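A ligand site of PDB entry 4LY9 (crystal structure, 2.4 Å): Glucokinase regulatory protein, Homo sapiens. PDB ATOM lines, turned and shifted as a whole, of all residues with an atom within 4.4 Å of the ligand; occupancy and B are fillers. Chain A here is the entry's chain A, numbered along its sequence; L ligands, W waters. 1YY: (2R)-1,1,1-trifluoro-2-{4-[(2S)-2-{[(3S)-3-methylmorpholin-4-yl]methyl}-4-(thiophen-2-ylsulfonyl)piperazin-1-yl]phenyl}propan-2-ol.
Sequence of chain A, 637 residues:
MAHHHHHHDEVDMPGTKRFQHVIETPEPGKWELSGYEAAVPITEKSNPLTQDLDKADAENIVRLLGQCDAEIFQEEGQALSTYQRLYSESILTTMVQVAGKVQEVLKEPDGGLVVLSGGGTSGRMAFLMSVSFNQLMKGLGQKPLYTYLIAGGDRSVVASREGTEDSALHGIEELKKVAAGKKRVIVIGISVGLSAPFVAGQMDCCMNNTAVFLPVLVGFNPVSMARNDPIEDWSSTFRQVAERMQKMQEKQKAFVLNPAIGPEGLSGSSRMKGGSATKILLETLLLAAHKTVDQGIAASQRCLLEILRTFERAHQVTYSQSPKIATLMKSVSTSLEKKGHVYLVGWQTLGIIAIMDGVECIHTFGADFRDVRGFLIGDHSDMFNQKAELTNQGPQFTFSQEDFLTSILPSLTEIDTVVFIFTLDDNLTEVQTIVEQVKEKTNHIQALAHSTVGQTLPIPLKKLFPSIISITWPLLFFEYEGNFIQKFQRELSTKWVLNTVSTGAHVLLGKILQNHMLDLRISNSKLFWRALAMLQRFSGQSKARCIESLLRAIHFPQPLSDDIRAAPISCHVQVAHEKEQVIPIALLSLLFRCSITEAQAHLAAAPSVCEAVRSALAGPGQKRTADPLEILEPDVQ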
ATOM      1  N   HIS A  21      -1.289   7.959 -11.920  1.00  0.00           N
ATOM      2  CA  HIS A  21      -0.286   7.378 -12.765  1.00  0.00           C
ATOM      3  C   HIS A  21       1.173   7.773 -12.370  1.00  0.00           C
ATOM      4  O   HIS A  21       2.131   7.199 -12.896  1.00  0.00           O
ATOM      5  CB  HIS A  21      -0.585   7.720 -14.214  1.00  0.00           C
ATOM      6  CG  HIS A  21       0.200   8.859 -14.772  1.00  0.00           C
ATOM      7  ND1 HIS A  21       0.020  10.163 -14.365  1.00  0.00           N
ATOM      8  CD2 HIS A  21       1.137   8.899 -15.757  1.00  0.00           C
ATOM      9  CE1 HIS A  21       0.837  10.949 -15.041  1.00  0.00           C
ATOM     10  NE2 HIS A  21       1.535  10.208 -15.892  1.00  0.00           N
ATOM     11  N   VAL A  22       1.351   8.721 -11.436  1.00  0.00           N
ATOM     12  CA  VAL A  22       2.686   9.134 -11.066  1.00  0.00           C
ATOM     13  C   VAL A  22       3.245   8.003 -10.228  1.00  0.00           C
ATOM     14  O   VAL A  22       2.613   7.609  -9.320  1.00  0.00           O
ATOM     15  CB  VAL A  22       2.713  10.441 -10.269  1.00  0.00           C
ATOM     16  CG1 VAL A  22       4.130  10.784  -9.887  1.00  0.00           C
ATOM     17  CG2 VAL A  22       2.160  11.567 -11.096  1.00  0.00           C
ATOM     18  N   ILE A  23       4.405   7.460 -10.599  1.00  0.00           N
ATOM     19  CA  ILE A  23       5.089   6.474  -9.786  1.00  0.00           C
ATOM     20  C   ILE A  23       5.759   7.173  -8.593  1.00  0.00           C
ATOM     21  O   ILE A  23       6.347   8.260  -8.749  1.00  0.00           O
ATOM     22  CB  ILE A  23       6.205   5.757 -10.585  1.00  0.00           C
ATOM     23  CG1 ILE A  23       5.696   5.124 -11.887  1.00  0.00           C
ATOM     24  CG2 ILE A  23       6.842   4.655  -9.754  1.00  0.00           C
ATOM     25  CD1 ILE A  23       4.802   3.917 -11.721  1.00  0.00           C
ATOM     26  N   TYR A  36      11.390   1.698 -11.083  1.00  0.00           N
ATOM     27  CA  TYR A  36      11.100   3.053 -11.545  1.00  0.00           C
ATOM     28  C   TYR A  36      11.799   3.264 -12.877  1.00  0.00           C
ATOM     29  O   TYR A  36      11.145   3.623 -13.842  1.00  0.00           O
ATOM     30  CB  TYR A  36      11.526   4.115 -10.538  1.00  0.00           C
ATOM     31  CG  TYR A  36      11.128   5.529 -10.890  1.00  0.00           C
ATOM     32  CD1 TYR A  36      11.853   6.290 -11.814  1.00  0.00           C
ATOM     33  CD2 TYR A  36      10.077   6.124 -10.286  1.00  0.00           C
ATOM     34  CE1 TYR A  36      11.520   7.586 -12.128  1.00  0.00           C
ATOM     35  CE2 TYR A  36       9.733   7.428 -10.590  1.00  0.00           C
ATOM     36  CZ  TYR A  36      10.455   8.161 -11.523  1.00  0.00           C
ATOM     37  OH  TYR A  36      10.078   9.455 -11.805  1.00  0.00           O
ATOM     38  N   VAL A  40      10.538   4.376 -17.025  1.00  0.00           N
ATOM     39  CA  VAL A  40      10.792   5.635 -17.732  1.00  0.00           C
ATOM     40  C   VAL A  40      10.881   5.340 -19.206  1.00  0.00           C
ATOM     41  O   VAL A  40      11.780   4.605 -19.647  1.00  0.00           O
ATOM     42  CB  VAL A  40      12.068   6.373 -17.282  1.00  0.00           C
ATOM     43  CG1 VAL A  40      12.195   7.720 -18.011  1.00  0.00           C
ATOM     44  CG2 VAL A  40      12.042   6.624 -15.757  1.00  0.00           C
ATOM     45  N   PRO A  41       9.947   5.913 -19.981  1.00  0.00           N
ATOM     46  CA  PRO A  41       9.985   5.727 -21.437  1.00  0.00           C
ATOM     47  C   PRO A  41      11.347   5.938 -22.033  1.00  0.00           C
ATOM     48  O   PRO A  41      12.068   6.855 -21.619  1.00  0.00           O
ATOM     49  CB  PRO A  41       8.989   6.777 -21.953  1.00  0.00           C
ATOM     50  CG  PRO A  41       8.042   6.999 -20.804  1.00  0.00           C
ATOM     51  CD  PRO A  41       8.893   6.872 -19.573  1.00  0.00           C
ATOM     52  N   THR A  43      12.277   7.499 -24.487  1.00  0.00           N
ATOM     53  CA  THR A  43      12.404   8.833 -24.999  1.00  0.00           C
ATOM     54  C   THR A  43      12.689   9.886 -23.922  1.00  0.00           C
ATOM     55  O   THR A  43      13.185  10.933 -24.231  1.00  0.00           O
ATOM     56  CB  THR A  43      11.137   9.255 -25.778  1.00  0.00           C
ATOM     57  OG1 THR A  43       9.935   9.175 -24.940  1.00  0.00           O
ATOM     58  CG2 THR A  43      11.020   8.357 -26.994  1.00  0.00           C
ATOM     59  N   GLU A  44      12.360   9.592 -22.680  1.00  0.00           N
ATOM     60  CA  GLU A  44      12.608  10.516 -21.572  1.00  0.00           C
ATOM     61  C   GLU A  44      13.824  10.203 -20.774  1.00  0.00           C
ATOM     62  O   GLU A  44      14.182  10.966 -19.875  1.00  0.00           O
ATOM     63  CB  GLU A  44      11.401  10.444 -20.625  1.00  0.00           C
ATOM     64  CG  GLU A  44      10.106  10.838 -21.330  1.00  0.00           C
ATOM     65  CD  GLU A  44       9.984  12.345 -21.650  1.00  0.00           C
ATOM     66  OE1 GLU A  44      10.576  13.121 -20.932  1.00  0.00           O
ATOM     67  OE2 GLU A  44       9.296  12.717 -22.625  1.00  0.00           O
ATOM     68  N   LYS A  45      14.471   9.096 -21.083  1.00  0.00           N
ATOM     69  CA  LYS A  45      15.560   8.630 -20.244  1.00  0.00           C
ATOM     70  C   LYS A  45      16.757   9.565 -20.267  1.00  0.00           C
ATOM     71  O   LYS A  45      16.932  10.312 -21.242  1.00  0.00           O
ATOM     72  CB  LYS A  45      15.989   7.199 -20.628  1.00  0.00           C
ATOM     73  CG  LYS A  45      15.152   6.055 -20.034  1.00  0.00           C
ATOM     74  CD  LYS A  45      15.850   4.696 -20.253  1.00  0.00           C
ATOM     75  CE  LYS A  45      14.919   3.487 -20.323  1.00  0.00           C
ATOM     76  NZ  LYS A  45      14.099   3.249 -19.086  1.00  0.00           N
ATOM     77  N   SER A  46      17.546   9.522 -19.182  1.00  0.00           N
ATOM     78  CA  SER A  46      18.888  10.131 -19.102  1.00  0.00           C
ATOM     79  C   SER A  46      19.855   9.279 -19.953  1.00  0.00           C
ATOM     80  O   SER A  46      20.052   8.096 -19.681  1.00  0.00           O
ATOM     81  CB  SER A  46      19.395  10.160 -17.641  1.00  0.00           C
ATOM     82  OG  SER A  46      20.712  10.696 -17.557  1.00  0.00           O
ATOM     83  N   GLY A 193       7.354  10.176 -28.770  1.00  0.00           N
ATOM     84  CA  GLY A 193       7.140   9.598 -27.459  1.00  0.00           C
ATOM     85  C   GLY A 193       5.922   8.742 -27.378  1.00  0.00           C
ATOM     86  O   GLY A 193       5.637   8.216 -26.299  1.00  0.00           O
ATOM     87  N   SER A 195       3.015   9.861 -27.581  1.00  0.00           N
ATOM     88  CA  SER A 195       2.614  10.747 -26.535  1.00  0.00           C
ATOM     89  C   SER A 195       1.512  11.733 -26.921  1.00  0.00           C
ATOM     90  O   SER A 195       0.702  12.009 -26.061  1.00  0.00           O
ATOM     91  CB  SER A 195       3.836  11.570 -26.100  1.00  0.00           C
ATOM     92  OG  SER A 195       3.403  12.748 -25.424  1.00  0.00           O
ATOM     93  N   ASN A 221       9.149   4.680 -28.884  1.00  0.00           N
ATOM     94  CA  ASN A 221       8.983   3.932 -27.631  1.00  0.00           C
ATOM     95  C   ASN A 221       8.319   2.628 -27.942  1.00  0.00           C
ATOM     96  O   ASN A 221       7.528   2.569 -28.824  1.00  0.00           O
ATOM     97  CB  ASN A 221       8.118   4.686 -26.636  1.00  0.00           C
ATOM     98  CG  ASN A 221       8.896   5.649 -25.808  1.00  0.00           C
ATOM     99  OD1 ASN A 221      10.026   5.369 -25.386  1.00  0.00           O
ATOM    100  ND2 ASN A 221       8.311   6.814 -25.573  1.00  0.00           N
ATOM    101  N   MET A 225       5.538   1.277 -23.329  1.00  0.00           N
ATOM    102  CA  MET A 225       5.897   2.534 -22.707  1.00  0.00           C
ATOM    103  C   MET A 225       5.150   3.674 -23.340  1.00  0.00           C
ATOM    104  O   MET A 225       5.508   4.859 -23.165  1.00  0.00           O
ATOM    105  CB  MET A 225       7.399   2.784 -22.837  1.00  0.00           C
ATOM    106  CG  MET A 225       8.288   1.813 -22.076  1.00  0.00           C
ATOM    107  SD  MET A 225       9.976   1.983 -22.626  1.00  0.00           S
ATOM    108  CE  MET A 225      10.885   1.179 -21.306  1.00  0.00           C
ATOM    109  N   ALA A 226       4.108   3.394 -24.102  1.00  0.00           N
ATOM    110  CA  ALA A 226       3.384   4.480 -24.683  1.00  0.00           C
ATOM    111  C   ALA A 226       2.731   5.215 -23.559  1.00  0.00           C
ATOM    112  O   ALA A 226       2.449   4.645 -22.517  1.00  0.00           O
ATOM    113  CB  ALA A 226       2.351   4.012 -25.675  1.00  0.00           C
ATOM    114  N   ARG A 227       2.481   6.494 -23.773  1.00  0.00           N
ATOM    115  CA  ARG A 227       1.860   7.363 -22.772  1.00  0.00           C
ATOM    116  C   ARG A 227       0.488   6.858 -22.366  1.00  0.00           C
ATOM    117  O   ARG A 227      -0.328   6.448 -23.220  1.00  0.00           O
ATOM    118  CB  ARG A 227       1.787   8.768 -23.304  1.00  0.00           C
ATOM    119  CG  ARG A 227       1.539   9.749 -22.268  1.00  0.00           C
ATOM    120  CD  ARG A 227       1.723  11.142 -22.806  1.00  0.00           C
ATOM    121  NE  ARG A 227       1.160  12.102 -21.881  1.00  0.00           N
ATOM    122  CZ  ARG A 227       1.061  13.402 -22.104  1.00  0.00           C
ATOM    123  NH1 ARG A 227       1.482  13.937 -23.240  1.00  0.00           N
ATOM    124  NH2 ARG A 227       0.531  14.180 -21.172  1.00  0.00           N
ATOM    125  N   ASP A 229      -1.405   8.467 -19.336  1.00  0.00           N
ATOM    126  CA  ASP A 229      -2.215   9.381 -18.493  1.00  0.00           C
ATOM    127  C   ASP A 229      -3.398   9.893 -19.286  1.00  0.00           C
ATOM    128  O   ASP A 229      -3.332   9.869 -20.507  1.00  0.00           O
ATOM    129  CB  ASP A 229      -1.387  10.551 -17.924  1.00  0.00           C
ATOM    130  CG  ASP A 229      -0.826  11.451 -19.019  1.00  0.00           C
ATOM    131  OD1 ASP A 229      -0.263  10.892 -19.955  1.00  0.00           O
ATOM    132  OD2 ASP A 229      -0.930  12.686 -18.954  1.00  0.00           O
ATOM    133  N   SER A 267      18.069  14.912 -22.304  1.00  0.00           N
ATOM    134  CA  SER A 267      16.914  14.147 -21.864  1.00  0.00           C
ATOM    135  C   SER A 267      15.599  14.743 -22.352  1.00  0.00           C
ATOM    136  O   SER A 267      15.292  15.874 -22.040  1.00  0.00           O
ATOM    137  CB  SER A 267      16.877  14.055 -20.351  1.00  0.00           C
ATOM    138  OG  SER A 267      18.083  13.510 -19.850  1.00  0.00           O
ATOM    139  N   HIS A 516      19.865  17.326 -18.259  1.00  0.00           N
ATOM    140  CA  HIS A 516      18.482  17.745 -18.107  1.00  0.00           C
ATOM    141  C   HIS A 516      18.380  19.263 -18.280  1.00  0.00           C
ATOM    142  O   HIS A 516      19.264  20.037 -17.816  1.00  0.00           O
ATOM    143  CB  HIS A 516      17.995  17.356 -16.698  1.00  0.00           C
ATOM    144  CG  HIS A 516      18.023  15.888 -16.429  1.00  0.00           C
ATOM    145  ND1 HIS A 516      17.257  14.981 -17.140  1.00  0.00           N
ATOM    146  CD2 HIS A 516      18.725  15.150 -15.540  1.00  0.00           C
ATOM    147  CE1 HIS A 516      17.469  13.769 -16.691  1.00  0.00           C
ATOM    148  NE2 HIS A 516      18.344  13.837 -15.708  1.00  0.00           N
ATOM    149  N   LYS A 526       2.800  16.943 -21.073  1.00  0.00           N
ATOM    150  CA  LYS A 526       4.072  16.227 -21.069  1.00  0.00           C
ATOM    151  C   LYS A 526       5.244  16.962 -20.338  1.00  0.00           C
ATOM    152  O   LYS A 526       5.973  16.379 -19.535  1.00  0.00           O
ATOM    153  CB  LYS A 526       4.442  15.890 -22.497  1.00  0.00           C
ATOM    154  CG  LYS A 526       5.740  15.127 -22.645  1.00  0.00           C
ATOM    155  CD  LYS A 526       5.956  14.810 -24.115  1.00  0.00           C
ATOM    156  CE  LYS A 526       6.196  16.057 -24.981  1.00  0.00           C
ATOM    157  NZ  LYS A 526       6.354  15.563 -26.382  1.00  0.00           N
ATOM    158  N   TRP A 529       4.653  16.832 -16.764  1.00  0.00           N
ATOM    159  CA  TRP A 529       5.125  15.566 -16.193  1.00  0.00           C
ATOM    160  C   TRP A 529       6.622  15.477 -16.149  1.00  0.00           C
ATOM    161  O   TRP A 529       7.169  14.902 -15.187  1.00  0.00           O
ATOM    162  CB  TRP A 529       4.566  14.351 -16.890  1.00  0.00           C
ATOM    163  CG  TRP A 529       3.080  14.264 -16.836  1.00  0.00           C
ATOM    164  CD1 TRP A 529       2.257  14.210 -17.903  1.00  0.00           C
ATOM    165  CD2 TRP A 529       2.237  14.228 -15.673  1.00  0.00           C
ATOM    166  NE1 TRP A 529       0.963  14.094 -17.498  1.00  0.00           N
ATOM    167  CE2 TRP A 529       0.911  14.113 -16.133  1.00  0.00           C
ATOM    168  CE3 TRP A 529       2.480  14.249 -14.295  1.00  0.00           C
ATOM    169  CZ2 TRP A 529      -0.182  14.036 -15.253  1.00  0.00           C
ATOM    170  CZ3 TRP A 529       1.384  14.184 -13.409  1.00  0.00           C
ATOM    171  CH2 TRP A 529       0.074  14.093 -13.894  1.00  0.00           C
ATOM    172  N   ARG A 530       7.291  16.016 -17.185  1.00  0.00           N
ATOM    173  CA  ARG A 530       8.758  16.038 -17.184  1.00  0.00           C
ATOM    174  C   ARG A 530       9.229  16.898 -15.996  1.00  0.00           C
ATOM    175  O   ARG A 530      10.193  16.573 -15.316  1.00  0.00           O
ATOM    176  CB  ARG A 530       9.338  16.545 -18.499  1.00  0.00           C
ATOM    177  CG  ARG A 530      10.881  16.523 -18.585  1.00  0.00           C
ATOM    178  CD  ARG A 530      11.366  16.806 -20.024  1.00  0.00           C
ATOM    179  NE  ARG A 530      10.677  15.981 -21.057  1.00  0.00           N
ATOM    180  CZ  ARG A 530      10.437  16.348 -22.307  1.00  0.00           C
ATOM    181  NH1 ARG A 530      10.764  17.550 -22.725  1.00  0.00           N
ATOM    182  NH2 ARG A 530       9.814  15.549 -23.153  1.00  0.00           N
ATOM    183  N   ALA A 533       8.869  14.811 -12.842  1.00  0.00           N
ATOM    184  CA  ALA A 533      10.001  13.869 -12.817  1.00  0.00           C
ATOM    185  C   ALA A 533      11.367  14.452 -12.452  1.00  0.00           C
ATOM    186  O   ALA A 533      12.197  13.790 -11.771  1.00  0.00           O
ATOM    187  CB  ALA A 533      10.143  13.236 -14.175  1.00  0.00           C
ATOM    188  N   MET A 534      11.658  15.635 -12.977  1.00  0.00           N
ATOM    189  CA  MET A 534      12.942  16.247 -12.640  1.00  0.00           C
ATOM    190  C   MET A 534      12.950  16.578 -11.147  1.00  0.00           C
ATOM    191  O   MET A 534      13.943  16.308 -10.453  1.00  0.00           O
ATOM    192  CB  MET A 534      13.239  17.450 -13.555  1.00  0.00           C
ATOM    193  CG  MET A 534      13.609  17.003 -14.956  1.00  0.00           C
ATOM    194  SD  MET A 534      14.075  18.349 -16.017  1.00  0.00           S
ATOM    195  CE  MET A 534      12.593  19.292 -15.987  1.00  0.00           C
ATOM    196  N   GLN A 536      11.451  14.853  -8.807  1.00  0.00           N
ATOM    197  CA  GLN A 536      11.721  13.601  -8.063  1.00  0.00           C
ATOM    198  C   GLN A 536      13.177  13.191  -8.168  1.00  0.00           C
ATOM    199  O   GLN A 536      13.751  12.754  -7.196  1.00  0.00           O
ATOM    200  CB  GLN A 536      10.884  12.436  -8.565  1.00  0.00           C
ATOM    201  CG  GLN A 536       9.386  12.665  -8.693  1.00  0.00           C
ATOM    202  CD  GLN A 536       8.719  11.434  -9.214  1.00  0.00           C
ATOM    203  OE1 GLN A 536       8.715  11.210 -10.420  1.00  0.00           O
ATOM    204  NE2 GLN A 536       8.274  10.553  -8.299  1.00  0.00           N
ATOM    205  N   ARG A 537      13.757  13.297  -9.360  1.00  0.00           N
ATOM    206  CA  ARG A 537      15.121  12.879  -9.587  1.00  0.00           C
ATOM    207  C   ARG A 537      16.168  13.743  -8.830  1.00  0.00           C
ATOM    208  O   ARG A 537      17.157  13.213  -8.388  1.00  0.00           O
ATOM    209  CB  ARG A 537      15.431  12.892 -11.080  1.00  0.00           C
ATOM    210  CG  ARG A 537      16.863  12.532 -11.504  1.00  0.00           C
ATOM    211  CD  ARG A 537      17.160  11.062 -11.373  1.00  0.00           C
ATOM    212  NE  ARG A 537      16.349  10.256 -12.286  1.00  0.00           N
ATOM    213  CZ  ARG A 537      16.510   8.948 -12.487  1.00  0.00           C
ATOM    214  NH1 ARG A 537      17.432   8.270 -11.796  1.00  0.00           N
ATOM    215  NH2 ARG A 537      15.734   8.316 -13.363  1.00  0.00           N
HETATM  216  C22 1YY L   1       6.277  11.639 -13.502  1.00  0.00           C
HETATM  217  C21 1YY L   1       7.146  10.379 -13.825  1.00  0.00           C
HETATM  218  C20 1YY L   1       6.904   9.267 -12.795  1.00  0.00           C
HETATM  219  O4  1YY L   1       5.592   8.681 -12.892  1.00  0.00           O
HETATM  220  C19 1YY L   1       5.165   8.285 -14.229  1.00  0.00           C
HETATM  221  C18 1YY L   1       5.434   9.461 -15.182  1.00  0.00           C
HETATM  222  N3  1YY L   1       6.850   9.821 -15.152  1.00  0.00           N
HETATM  223  C5  1YY L   1       7.171  10.803 -16.208  1.00  0.00           C
HETATM  224  C3  1YY L   1       7.817  10.219 -17.476  1.00  0.00           C
HETATM  225  C2  1YY L   1       6.754  10.136 -18.622  1.00  0.00           C
HETATM  226  N1  1YY L   1       6.043  11.422 -18.793  1.00  0.00           N
HETATM  227  S1  1YY L   1       4.748  11.264 -19.732  1.00  0.00           S
HETATM  228  O1  1YY L   1       4.327  12.613 -20.207  1.00  0.00           O
HETATM  229  O2  1YY L   1       3.758  10.479 -18.940  1.00  0.00           O
HETATM  230  C6  1YY L   1       5.105  10.319 -21.143  1.00  0.00           C
HETATM  231  C7  1YY L   1       4.904   9.000 -21.304  1.00  0.00           C
HETATM  232  C8  1YY L   1       5.334   8.558 -22.497  1.00  0.00           C
HETATM  233  C9  1YY L   1       5.886   9.475 -23.341  1.00  0.00           C
HETATM  234  S2  1YY L   1       5.793  10.972 -22.524  1.00  0.00           S
HETATM  235  C1  1YY L   1       7.031  12.277 -19.403  1.00  0.00           C
HETATM  236  C4  1YY L   1       8.307  12.378 -18.569  1.00  0.00           C
HETATM  237  N2  1YY L   1       8.751  11.216 -17.847  1.00  0.00           N
HETATM  238  C10 1YY L   1       9.999  11.257 -17.226  1.00  0.00           C
HETATM  239  C15 1YY L   1      10.904  12.251 -17.556  1.00  0.00           C
HETATM  240  C14 1YY L   1      12.148  12.325 -16.971  1.00  0.00           C
HETATM  241  C11 1YY L   1      10.386  10.322 -16.292  1.00  0.00           C
HETATM  242  C12 1YY L   1      11.629  10.368 -15.682  1.00  0.00           C
HETATM  243  C13 1YY L   1      12.503  11.363 -16.029  1.00  0.00           C
HETATM  244  C16 1YY L   1      13.845  11.469 -15.367  1.00  0.00           C
HETATM  245  C23 1YY L   1      14.996  11.029 -16.218  1.00  0.00           C
HETATM  246  F2  1YY L   1      16.129  10.957 -15.487  1.00  0.00           F
HETATM  247  F3  1YY L   1      15.138  11.921 -17.239  1.00  0.00           F
HETATM  248  F1  1YY L   1      14.720   9.812 -16.598  1.00  0.00           F
HETATM  249  C17 1YY L   1      14.031  12.960 -15.124  1.00  0.00           C
HETATM  250  O3  1YY L   1      13.826  10.722 -14.181  1.00  0.00           O
HETATM  251  O   HOH W   1       8.503  11.403 -24.589  1.00  0.00           O
HETATM  252  O   HOH W   2       2.471   7.803 -18.624  1.00  0.00           O
HETATM  253  O   HOH W   3      13.177  13.460 -20.105  1.00  0.00           O
HETATM  254  O   HOH W   4      12.202  11.109 -12.162  1.00  0.00           O
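O of Glu 44 sits close to F3 of the ligand.
Residues that only touch the ligand: His 516, Gly 193, Tyr 36, Val 22, Trp 529, His 21, Ala 533, Pro 41, Gln 536, Val 40, Arg 227, Lys 526, Met 225, Ser 46, Lys 45 and Arg 530.
Hydrophobic or aromatic side chains that line the ligand: Val 22, Ile 23, Tyr 36, Val 40, Pro 41, His 516, Trp 529 and Ala 533.
Within 4 Å of the ligand: His 21, Val 22, Ile 23, Tyr 36, Val 40, Pro 41, Glu 44, Lys 45, Ser 46, Gly 193, Met 225, Arg 227, His 516, Lys 526, Trp 529, Arg 530, Ala 533, Gln 536 and Arg 537.
Along chain A the residues within 4 Å of the ligand span positions 21 to 537.
A ring nitrogen (ND1) of His 516 lies within hydrogen-bond range of the side-chain hydroxyl of Ser 267 (3.2 Å).
OE1 of Glu 44 is in salt-bridge range of NE of Arg 530 (2.9 Å).
The side-chain hydroxyl (OG) of Ser 195 is in hydrogen-bond range of the guanidinium group (NH1) of Arg 227.
The indole nitrogen (NE1) of Trp 529 lies within hydrogen-bond range of the side-chain carboxylate (OD2) of Asp 229, 2.8 Å away.
The backbone carbonyl oxygen (O) of Gly 193 is in hydrogen-bond range of the side-chain amide nitrogen (ND2) of Asn 221 (3.1 Å).
NZ of Lys 45 lies within hydrogen-bond range of O of Val 40.
OE1 of Gln 536 sits at hydrogen-bond distance from OH of Tyr 36 (2.6 Å).
NE of Arg 227 lies within salt-bridge range of OD1 of Asp 229, at 2.7 Å.
NH2 of Arg 537 is in hydrogen-bond range of O3 of the ligand (3.2 Å).
An oxygen (O4) of the ligand sits at hydrogen-bond distance from the backbone NH (N) of Ile 23 (2.9 Å).
Water W4 lies within hydrogen-bond range of an oxygen (O3) of the ligand (2.6 Å), the backbone carbonyl oxygen of Ala 533 (2.7 Å) and the side-chain hydroxyl of Tyr 36 (2.7 Å).
Water W1 lies within hydrogen-bond range of the side-chain carboxylate (OE2) of Glu 44, the side-chain hydroxyl (OG1) of Thr 43 and a sulfur (S2) of the ligand.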
